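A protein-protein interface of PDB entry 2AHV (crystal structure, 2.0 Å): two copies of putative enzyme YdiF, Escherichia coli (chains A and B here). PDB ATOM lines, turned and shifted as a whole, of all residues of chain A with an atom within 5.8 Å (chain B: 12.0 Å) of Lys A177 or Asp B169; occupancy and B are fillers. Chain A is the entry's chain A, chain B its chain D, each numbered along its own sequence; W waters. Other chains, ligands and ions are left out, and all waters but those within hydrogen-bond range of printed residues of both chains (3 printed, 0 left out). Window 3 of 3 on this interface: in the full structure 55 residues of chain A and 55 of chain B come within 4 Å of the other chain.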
ATOM      1  N   TYR A 116     -14.884 -13.439  28.433  1.00  0.00           N
ATOM      2  CA  TYR A 116     -13.695 -13.501  27.583  1.00  0.00           C
ATOM      3  C   TYR A 116     -13.398 -12.052  27.205  1.00  0.00           C
ATOM      4  O   TYR A 116     -14.331 -11.243  27.116  1.00  0.00           O
ATOM      5  CB  TYR A 116     -13.982 -14.256  26.271  1.00  0.00           C
ATOM      6  CG  TYR A 116     -13.962 -15.782  26.258  1.00  0.00           C
ATOM      7  CD1 TYR A 116     -13.899 -16.541  27.434  1.00  0.00           C
ATOM      8  CD2 TYR A 116     -14.052 -16.466  25.039  1.00  0.00           C
ATOM      9  CE1 TYR A 116     -13.904 -17.958  27.380  1.00  0.00           C
ATOM     10  CE2 TYR A 116     -14.053 -17.862  24.979  1.00  0.00           C
ATOM     11  CZ  TYR A 116     -13.973 -18.600  26.150  1.00  0.00           C
ATOM     12  OH  TYR A 116     -13.988 -19.971  26.078  1.00  0.00           O
ATOM     13  N   THR A 124     -12.981 -16.184  18.740  1.00  0.00           N
ATOM     14  CA  THR A 124     -13.415 -17.570  18.970  1.00  0.00           C
ATOM     15  C   THR A 124     -14.674 -17.914  18.182  1.00  0.00           C
ATOM     16  O   THR A 124     -14.856 -19.058  17.784  1.00  0.00           O
ATOM     17  CB  THR A 124     -13.624 -17.920  20.457  1.00  0.00           C
ATOM     18  OG1 THR A 124     -14.621 -17.064  21.042  1.00  0.00           O
ATOM     19  CG2 THR A 124     -12.332 -17.727  21.262  1.00  0.00           C
ATOM     20  N   PRO A 133     -11.297 -25.726  17.329  1.00  0.00           N
ATOM     21  CA  PRO A 133     -11.753 -26.009  18.693  1.00  0.00           C
ATOM     22  C   PRO A 133     -11.562 -24.845  19.673  1.00  0.00           C
ATOM     23  O   PRO A 133     -12.321 -24.722  20.645  1.00  0.00           O
ATOM     24  CB  PRO A 133     -10.903 -27.221  19.094  1.00  0.00           C
ATOM     25  CG  PRO A 133      -9.653 -27.044  18.350  1.00  0.00           C
ATOM     26  CD  PRO A 133     -10.039 -26.427  17.020  1.00  0.00           C
ATOM     27  N   GLY A 134     -10.577 -23.993  19.402  1.00  0.00           N
ATOM     28  CA  GLY A 134     -10.293 -22.821  20.238  1.00  0.00           C
ATOM     29  C   GLY A 134      -9.186 -21.977  19.640  1.00  0.00           C
ATOM     30  O   GLY A 134      -8.703 -22.271  18.551  1.00  0.00           O
ATOM     31  N   ILE A 135      -8.793 -20.910  20.335  1.00  0.00           N
ATOM     32  CA  ILE A 135      -7.659 -20.102  19.877  1.00  0.00           C
ATOM     33  C   ILE A 135      -6.571 -19.988  20.946  1.00  0.00           C
ATOM     34  O   ILE A 135      -6.864 -19.992  22.148  1.00  0.00           O
ATOM     35  CB  ILE A 135      -8.090 -18.678  19.390  1.00  0.00           C
ATOM     36  CG1 ILE A 135      -8.366 -17.756  20.562  1.00  0.00           C
ATOM     37  CG2 ILE A 135      -9.269 -18.714  18.363  1.00  0.00           C
ATOM     38  CD1 ILE A 135      -8.253 -16.301  20.202  1.00  0.00           C
ATOM     39  N   GLU A 160     -17.183 -24.714  35.262  1.00  0.00           N
ATOM     40  CA  GLU A 160     -16.530 -25.344  34.105  1.00  0.00           C
ATOM     41  C   GLU A 160     -15.396 -24.483  33.544  1.00  0.00           C
ATOM     42  O   GLU A 160     -15.580 -23.292  33.312  1.00  0.00           O
ATOM     43  CB  GLU A 160     -17.573 -25.628  33.025  1.00  0.00           C
ATOM     44  CG  GLU A 160     -17.082 -26.423  31.828  1.00  0.00           C
ATOM     45  CD  GLU A 160     -18.216 -26.778  30.880  1.00  0.00           C
ATOM     46  OE1 GLU A 160     -19.285 -27.243  31.368  1.00  0.00           O
ATOM     47  OE2 GLU A 160     -18.046 -26.592  29.648  1.00  0.00           O
ATOM     48  N   ASP A 161     -14.228 -25.091  33.342  1.00  0.00           N
ATOM     49  CA  ASP A 161     -13.086 -24.404  32.748  1.00  0.00           C
ATOM     50  C   ASP A 161     -13.312 -24.256  31.251  1.00  0.00           C
ATOM     51  O   ASP A 161     -13.556 -25.247  30.564  1.00  0.00           O
ATOM     52  CB  ASP A 161     -11.788 -25.193  32.974  1.00  0.00           C
ATOM     53  CG  ASP A 161     -11.442 -25.367  34.447  1.00  0.00           C
ATOM     54  OD1 ASP A 161     -11.559 -24.397  35.230  1.00  0.00           O
ATOM     55  OD2 ASP A 161     -11.018 -26.449  34.904  1.00  0.00           O
ATOM     56  N   LEU A 162     -13.242 -23.028  30.751  1.00  0.00           N
ATOM     57  CA  LEU A 162     -13.264 -22.789  29.304  1.00  0.00           C
ATOM     58  C   LEU A 162     -11.907 -22.339  28.793  1.00  0.00           C
ATOM     59  O   LEU A 162     -11.640 -22.377  27.595  1.00  0.00           O
ATOM     60  CB  LEU A 162     -14.296 -21.725  28.940  1.00  0.00           C
ATOM     61  CG  LEU A 162     -15.774 -22.014  29.159  1.00  0.00           C
ATOM     62  CD1 LEU A 162     -16.566 -20.830  28.643  1.00  0.00           C
ATOM     63  CD2 LEU A 162     -16.208 -23.321  28.481  1.00  0.00           C
ATOM     64  N   ILE A 163     -11.073 -21.858  29.710  1.00  0.00           N
ATOM     65  CA  ILE A 163      -9.744 -21.371  29.372  1.00  0.00           C
ATOM     66  C   ILE A 163      -8.684 -22.234  30.052  1.00  0.00           C
ATOM     67  O   ILE A 163      -8.811 -22.583  31.230  1.00  0.00           O
ATOM     68  CB  ILE A 163      -9.581 -19.898  29.770  1.00  0.00           C
ATOM     69  CG1 ILE A 163     -10.737 -19.068  29.216  1.00  0.00           C
ATOM     70  CG2 ILE A 163      -8.215 -19.363  29.292  1.00  0.00           C
ATOM     71  CD1 ILE A 163     -10.856 -17.726  29.829  1.00  0.00           C
ATOM     72  N   LYS A 164      -7.644 -22.549  29.292  1.00  0.00           N
ATOM     73  CA  LYS A 164      -6.633 -23.510  29.682  1.00  0.00           C
ATOM     74  C   LYS A 164      -5.274 -22.882  29.411  1.00  0.00           C
ATOM     75  O   LYS A 164      -5.095 -22.178  28.418  1.00  0.00           O
ATOM     76  CB  LYS A 164      -6.845 -24.798  28.860  1.00  0.00           C
ATOM     77  CG  LYS A 164      -5.754 -25.841  28.909  1.00  0.00           C
ATOM     78  CD  LYS A 164      -6.283 -27.201  28.448  1.00  0.00           C
ATOM     79  CE  LYS A 164      -6.320 -27.336  26.925  1.00  0.00           C
ATOM     80  NZ  LYS A 164      -7.058 -28.574  26.498  1.00  0.00           N
ATOM     81  N   TYR A 175      -5.447 -20.862  26.041  1.00  0.00           N
ATOM     82  CA  TYR A 175      -6.293 -21.517  25.063  1.00  0.00           C
ATOM     83  C   TYR A 175      -7.741 -21.249  25.448  1.00  0.00           C
ATOM     84  O   TYR A 175      -8.194 -21.659  26.518  1.00  0.00           O
ATOM     85  CB  TYR A 175      -6.008 -23.022  25.017  1.00  0.00           C
ATOM     86  CG  TYR A 175      -7.004 -23.817  24.205  1.00  0.00           C
ATOM     87  CD1 TYR A 175      -6.890 -23.903  22.815  1.00  0.00           C
ATOM     88  CD2 TYR A 175      -8.066 -24.481  24.821  1.00  0.00           C
ATOM     89  CE1 TYR A 175      -7.812 -24.627  22.062  1.00  0.00           C
ATOM     90  CE2 TYR A 175      -8.993 -25.209  24.069  1.00  0.00           C
ATOM     91  CZ  TYR A 175      -8.853 -25.269  22.692  1.00  0.00           C
ATOM     92  OH  TYR A 175      -9.755 -25.993  21.944  1.00  0.00           O
ATOM     93  N   TYR A 176      -8.457 -20.546  24.578  1.00  0.00           N
ATOM     94  CA  TYR A 176      -9.839 -20.210  24.825  1.00  0.00           C
ATOM     95  C   TYR A 176     -10.722 -21.114  23.984  1.00  0.00           C
ATOM     96  O   TYR A 176     -10.618 -21.102  22.763  1.00  0.00           O
ATOM     97  CB  TYR A 176     -10.125 -18.785  24.379  1.00  0.00           C
ATOM     98  CG  TYR A 176      -9.481 -17.671  25.159  1.00  0.00           C
ATOM     99  CD1 TYR A 176     -10.205 -16.985  26.140  1.00  0.00           C
ATOM    100  CD2 TYR A 176      -8.189 -17.251  24.869  1.00  0.00           C
ATOM    101  CE1 TYR A 176      -9.634 -15.924  26.843  1.00  0.00           C
ATOM    102  CE2 TYR A 176      -7.602 -16.179  25.566  1.00  0.00           C
ATOM    103  CZ  TYR A 176      -8.333 -15.520  26.541  1.00  0.00           C
ATOM    104  OH  TYR A 176      -7.763 -14.456  27.220  1.00  0.00           O
ATOM    105  N   LYS A 177     -11.617 -21.858  24.625  1.00  0.00           N
ATOM    106  CA  LYS A 177     -12.507 -22.762  23.897  1.00  0.00           C
ATOM    107  C   LYS A 177     -13.462 -21.965  22.993  1.00  0.00           C
ATOM    108  O   LYS A 177     -14.036 -20.970  23.425  1.00  0.00           O
ATOM    109  CB  LYS A 177     -13.293 -23.630  24.882  1.00  0.00           C
ATOM    110  CG  LYS A 177     -14.207 -24.656  24.217  1.00  0.00           C
ATOM    111  CD  LYS A 177     -15.077 -25.375  25.252  1.00  0.00           C
ATOM    112  CE  LYS A 177     -15.892 -26.504  24.625  1.00  0.00           C
ATOM    113  NZ  LYS A 177     -14.988 -27.518  24.000  1.00  0.00           N
ATOM    114  N   ALA A 178     -13.600 -22.399  21.739  1.00  0.00           N
ATOM    115  CA  ALA A 178     -14.516 -21.762  20.787  1.00  0.00           C
ATOM    116  C   ALA A 178     -15.897 -22.385  20.918  1.00  0.00           C
ATOM    117  O   ALA A 178     -16.057 -23.602  20.821  1.00  0.00           O
ATOM    118  CB  ALA A 178     -13.984 -21.887  19.357  1.00  0.00           C
ATOM    119  N   ILE A 179     -16.893 -21.554  21.192  1.00  0.00           N
ATOM    120  CA  ILE A 179     -18.260 -22.033  21.385  1.00  0.00           C
ATOM    121  C   ILE A 179     -19.101 -21.517  20.225  1.00  0.00           C
ATOM    122  O   ILE A 179     -19.091 -20.317  19.928  1.00  0.00           O
ATOM    123  CB  ILE A 179     -18.824 -21.562  22.751  1.00  0.00           C
ATOM    124  CG1 ILE A 179     -17.985 -22.137  23.897  1.00  0.00           C
ATOM    125  CG2 ILE A 179     -20.294 -22.010  22.929  1.00  0.00           C
ATOM    126  CD1 ILE A 179     -18.246 -21.488  25.224  1.00  0.00           C
ATOM    127  N   GLN B 132      -0.664 -14.427  17.459  1.00  0.00           N
ATOM    128  CA  GLN B 132      -0.993 -15.797  17.849  1.00  0.00           C
ATOM    129  C   GLN B 132       0.084 -16.710  17.242  1.00  0.00           C
ATOM    130  O   GLN B 132       0.495 -16.486  16.108  1.00  0.00           O
ATOM    131  CB  GLN B 132      -2.405 -16.168  17.375  1.00  0.00           C
ATOM    132  CG  GLN B 132      -3.492 -15.320  18.045  1.00  0.00           C
ATOM    133  CD  GLN B 132      -4.893 -15.583  17.513  1.00  0.00           C
ATOM    134  OE1 GLN B 132      -5.111 -16.519  16.734  1.00  0.00           O
ATOM    135  NE2 GLN B 132      -5.851 -14.774  17.958  1.00  0.00           N
ATOM    136  N   ILE B 136      -5.101 -24.095  15.288  1.00  0.00           N
ATOM    137  CA  ILE B 136      -5.505 -25.478  15.478  1.00  0.00           C
ATOM    138  C   ILE B 136      -6.648 -25.781  14.538  1.00  0.00           C
ATOM    139  O   ILE B 136      -7.690 -25.129  14.580  1.00  0.00           O
ATOM    140  CB  ILE B 136      -5.956 -25.699  16.919  1.00  0.00           C
ATOM    141  CG1 ILE B 136      -4.905 -25.132  17.886  1.00  0.00           C
ATOM    142  CG2 ILE B 136      -6.245 -27.182  17.171  1.00  0.00           C
ATOM    143  CD1 ILE B 136      -5.428 -24.900  19.278  1.00  0.00           C
ATOM    144  N   SER B 137      -6.450 -26.790  13.702  1.00  0.00           N
ATOM    145  CA  SER B 137      -7.441 -27.146  12.703  1.00  0.00           C
ATOM    146  C   SER B 137      -7.332 -28.624  12.371  1.00  0.00           C
ATOM    147  O   SER B 137      -6.233 -29.177  12.341  1.00  0.00           O
ATOM    148  CB  SER B 137      -7.208 -26.316  11.443  1.00  0.00           C
ATOM    149  OG  SER B 137      -8.024 -26.781  10.383  1.00  0.00           O
ATOM    150  N   ASP B 138      -8.464 -29.262  12.100  1.00  0.00           N
ATOM    151  CA  ASP B 138      -8.423 -30.650  11.638  1.00  0.00           C
ATOM    152  C   ASP B 138      -8.315 -30.730  10.117  1.00  0.00           C
ATOM    153  O   ASP B 138      -8.252 -31.820   9.544  1.00  0.00           O
ATOM    154  CB  ASP B 138      -9.603 -31.471  12.174  1.00  0.00           C
ATOM    155  CG  ASP B 138     -10.940 -30.951  11.712  1.00  0.00           C
ATOM    156  OD1 ASP B 138     -11.023 -30.265  10.670  1.00  0.00           O
ATOM    157  OD2 ASP B 138     -11.988 -31.207  12.332  1.00  0.00           O
ATOM    158  N   LEU B 165       1.100 -32.390  15.532  1.00  0.00           N
ATOM    159  CA  LEU B 165      -0.149 -33.033  15.924  1.00  0.00           C
ATOM    160  C   LEU B 165      -0.442 -32.719  17.384  1.00  0.00           C
ATOM    161  O   LEU B 165       0.440 -32.838  18.229  1.00  0.00           O
ATOM    162  CB  LEU B 165      -0.057 -34.547  15.687  1.00  0.00           C
ATOM    163  CG  LEU B 165      -1.258 -35.468  15.888  1.00  0.00           C
ATOM    164  CD1 LEU B 165      -2.370 -35.241  14.852  1.00  0.00           C
ATOM    165  CD2 LEU B 165      -0.749 -36.902  15.825  1.00  0.00           C
ATOM    166  N   VAL B 166      -1.675 -32.295  17.668  1.00  0.00           N
ATOM    167  CA  VAL B 166      -2.094 -31.903  19.017  1.00  0.00           C
ATOM    168  C   VAL B 166      -3.432 -32.548  19.388  1.00  0.00           C
ATOM    169  O   VAL B 166      -4.100 -33.139  18.535  1.00  0.00           O
ATOM    170  CB  VAL B 166      -2.197 -30.353  19.183  1.00  0.00           C
ATOM    171  CG1 VAL B 166      -0.856 -29.674  18.947  1.00  0.00           C
ATOM    172  CG2 VAL B 166      -3.289 -29.760  18.267  1.00  0.00           C
ATOM    173  N   GLU B 167      -3.819 -32.426  20.659  1.00  0.00           N
ATOM    174  CA  GLU B 167      -5.075 -33.000  21.143  1.00  0.00           C
ATOM    175  C   GLU B 167      -5.890 -32.020  21.987  1.00  0.00           C
ATOM    176  O   GLU B 167      -5.366 -31.384  22.897  1.00  0.00           O
ATOM    177  CB  GLU B 167      -4.801 -34.269  21.944  1.00  0.00           C
ATOM    178  CG  GLU B 167      -5.975 -35.232  21.982  1.00  0.00           C
ATOM    179  CD  GLU B 167      -5.696 -36.448  22.847  1.00  0.00           C
ATOM    180  OE1 GLU B 167      -5.515 -37.560  22.285  1.00  0.00           O
ATOM    181  OE2 GLU B 167      -5.646 -36.282  24.088  1.00  0.00           O
ATOM    182  N   PHE B 168      -7.172 -31.908  21.655  1.00  0.00           N
ATOM    183  CA  PHE B 168      -8.141 -31.094  22.391  1.00  0.00           C
ATOM    184  C   PHE B 168      -9.488 -31.805  22.326  1.00  0.00           C
ATOM    185  O   PHE B 168      -9.857 -32.345  21.277  1.00  0.00           O
ATOM    186  CB  PHE B 168      -8.275 -29.698  21.772  1.00  0.00           C
ATOM    187  CG  PHE B 168      -7.069 -28.815  21.971  1.00  0.00           C
ATOM    188  CD1 PHE B 168      -6.932 -28.040  23.120  1.00  0.00           C
ATOM    189  CD2 PHE B 168      -6.082 -28.736  20.999  1.00  0.00           C
ATOM    190  CE1 PHE B 168      -5.823 -27.216  23.302  1.00  0.00           C
ATOM    191  CE2 PHE B 168      -4.967 -27.915  21.173  1.00  0.00           C
ATOM    192  CZ  PHE B 168      -4.839 -27.155  22.329  1.00  0.00           C
ATOM    193  N   ASP B 169     -10.220 -31.804  23.439  1.00  0.00           N
ATOM    194  CA  ASP B 169     -11.529 -32.490  23.539  1.00  0.00           C
ATOM    195  C   ASP B 169     -11.449 -33.952  23.112  1.00  0.00           C
ATOM    196  O   ASP B 169     -12.400 -34.478  22.522  1.00  0.00           O
ATOM    197  CB  ASP B 169     -12.608 -31.804  22.676  1.00  0.00           C
ATOM    198  CG  ASP B 169     -12.751 -30.321  22.963  1.00  0.00           C
ATOM    199  OD1 ASP B 169     -12.992 -29.957  24.140  1.00  0.00           O
ATOM    200  OD2 ASP B 169     -12.665 -29.452  22.059  1.00  0.00           O
ATOM    201  N   ASN B 170     -10.312 -34.598  23.377  1.00  0.00           N
ATOM    202  CA  ASN B 170     -10.094 -35.982  22.953  1.00  0.00           C
ATOM    203  C   ASN B 170     -10.146 -36.191  21.441  1.00  0.00           C
ATOM    204  O   ASN B 170     -10.457 -37.295  20.976  1.00  0.00           O
ATOM    205  CB  ASN B 170     -11.106 -36.918  23.630  1.00  0.00           C
ATOM    206  CG  ASN B 170     -10.565 -37.546  24.887  1.00  0.00           C
ATOM    207  OD1 ASN B 170     -10.331 -36.866  25.894  1.00  0.00           O
ATOM    208  ND2 ASN B 170     -10.366 -38.863  24.843  1.00  0.00           N
ATOM    209  N   LYS B 171      -9.866 -35.135  20.673  1.00  0.00           N
ATOM    210  CA  LYS B 171      -9.828 -35.243  19.210  1.00  0.00           C
ATOM    211  C   LYS B 171      -8.476 -34.817  18.664  1.00  0.00           C
ATOM    212  O   LYS B 171      -7.750 -34.064  19.307  1.00  0.00           O
ATOM    213  CB  LYS B 171     -10.944 -34.426  18.545  1.00  0.00           C
ATOM    214  CG  LYS B 171     -12.366 -34.788  18.994  1.00  0.00           C
ATOM    215  CD  LYS B 171     -13.360 -34.813  17.837  1.00  0.00           C
ATOM    216  CE  LYS B 171     -13.488 -33.472  17.100  1.00  0.00           C
ATOM    217  NZ  LYS B 171     -12.634 -33.359  15.858  1.00  0.00           N
ATOM    218  N   GLU B 172      -8.153 -35.309  17.474  1.00  0.00           N
ATOM    219  CA  GLU B 172      -6.907 -34.970  16.803  1.00  0.00           C
ATOM    220  C   GLU B 172      -7.083 -33.682  16.028  1.00  0.00           C
ATOM    221  O   GLU B 172      -8.104 -33.481  15.359  1.00  0.00           O
ATOM    222  CB  GLU B 172      -6.520 -36.049  15.788  1.00  0.00           C
ATOM    223  CG  GLU B 172      -5.873 -37.301  16.348  1.00  0.00           C
ATOM    224  CD  GLU B 172      -5.690 -38.368  15.279  1.00  0.00           C
ATOM    225  OE1 GLU B 172      -5.862 -38.053  14.070  1.00  0.00           O
ATOM    226  OE2 GLU B 172      -5.378 -39.527  15.649  1.00  0.00           O
ATOM    227  N   TYR B 173      -6.072 -32.824  16.103  1.00  0.00           N
ATOM    228  CA  TYR B 173      -6.015 -31.627  15.273  1.00  0.00           C
ATOM    229  C   TYR B 173      -4.575 -31.396  14.871  1.00  0.00           C
ATOM    230  O   TYR B 173      -3.656 -31.884  15.531  1.00  0.00           O
ATOM    231  CB  TYR B 173      -6.499 -30.402  16.042  1.00  0.00           C
ATOM    232  CG  TYR B 173      -7.907 -30.475  16.571  1.00  0.00           C
ATOM    233  CD1 TYR B 173      -8.990 -30.154  15.763  1.00  0.00           C
ATOM    234  CD2 TYR B 173      -8.155 -30.840  17.889  1.00  0.00           C
ATOM    235  CE1 TYR B 173     -10.284 -30.212  16.246  1.00  0.00           C
ATOM    236  CE2 TYR B 173      -9.455 -30.898  18.386  1.00  0.00           C
ATOM    237  CZ  TYR B 173     -10.512 -30.583  17.550  1.00  0.00           C
ATOM    238  OH  TYR B 173     -11.811 -30.636  18.013  1.00  0.00           O
ATOM    239  N   LEU B 174      -4.375 -30.639  13.797  1.00  0.00           N
ATOM    240  CA  LEU B 174      -3.049 -30.167  13.446  1.00  0.00           C
ATOM    241  C   LEU B 174      -2.867 -28.752  13.961  1.00  0.00           C
ATOM    242  O   LEU B 174      -3.801 -27.958  13.970  1.00  0.00           O
ATOM    243  CB  LEU B 174      -2.839 -30.182  11.932  1.00  0.00           C
ATOM    244  CG  LEU B 174      -2.994 -31.530  11.226  1.00  0.00           C
ATOM    245  CD1 LEU B 174      -2.545 -31.401   9.794  1.00  0.00           C
ATOM    246  CD2 LEU B 174      -2.185 -32.612  11.953  1.00  0.00           C
HETATM  247  O   HOH W   1     -13.943 -26.544  21.353  1.00  0.00           O
HETATM  248  O   HOH W   2     -11.454 -27.440  23.413  1.00  0.00           O
HETATM  249  O   HOH W   3      -6.999 -21.929  16.413  1.00  0.00           O
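OD1 of Asp B169 lies within salt-bridge range of NZ of Lys A177 (3.2 Å).
N of Tyr A176 is in hydrogen-bond range of O of Ile A135. O of Lys A164 sits at hydrogen-bond distance from N of Tyr A175. OH of Tyr A116 lies within hydrogen-bond range of O of Lys A177 (2.8 Å). The backbone carbonyl oxygen (O) of Leu A162 lies within hydrogen-bond range of the backbone NH (N) of Lys A177, at 3.0 Å. N of Ala A178 lies within hydrogen-bond range of O of Pro A133 (2.9 Å). OH of Tyr A175 sits at hydrogen-bond distance from N of Gly A134, 3.3 Å away.
Pro A133 touches Ile B136 (CG to CG2, 3.6 Å). OH of Tyr B173 touches CB of Pro A133, at 3.7 Å. Ile A135 touches Gln B132 (CD1 to NE2, 3.6 Å). CD1 of Phe B168 touches NZ of Lys A164, 3.4 Å away. Tyr A175 touches Ile B136. Tyr A175 touches Phe B168.
Lys A177 touches just one residue of chain B: Asp B169. Of the printed residues of chain B, Pro A133 touches Ile B136 and Tyr B173. No residue of chain B comes within 4 Å of Gly A134. Of chain B, only Gln B132 comes within 4 Å of Ile A135. Leu A162 touches none of the printed residues of chain B. No residue of chain B comes within 4 Å of Ala A178. No residue of chain B comes within 4 Å of Ile A179. Printed residues of chain A within 4 Å of Phe B168: Lys A164 (3.4 Å) and Tyr A175 (3.4 Å). Of the printed residues of chain B, Lys A164 touches Phe B168 (3.4 Å). Ser B137 touches none of the printed residues of chain A. The nearest residue of chain B that does not touch Lys A177 is Phe B168 (7.2 Å).
Hydrophobic or aromatic side chains of chain B that line the printed part of chain A: Ile B136, Phe B168 and Tyr B173. Among the printed residues, 7 pairs touch across the chains.
No position is printed for both chains.
Water W1 lies within hydrogen-bond range of the backbone carbonyl oxygen (O) of Pro A133 (2.5 Å), the side-chain amino group (NZ) of Lys A177 (3.0 Å) and the side-chain carboxylate (OD2) of Asp B169 (3.3 Å). Water W2 bridges OH of Tyr A175 (2.7 Å) and OD2 of Asp B169 (2.7 Å). Water W3 bridges O of Gly A134 (2.8 Å) and N of Ile B136 (3.1 Å).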
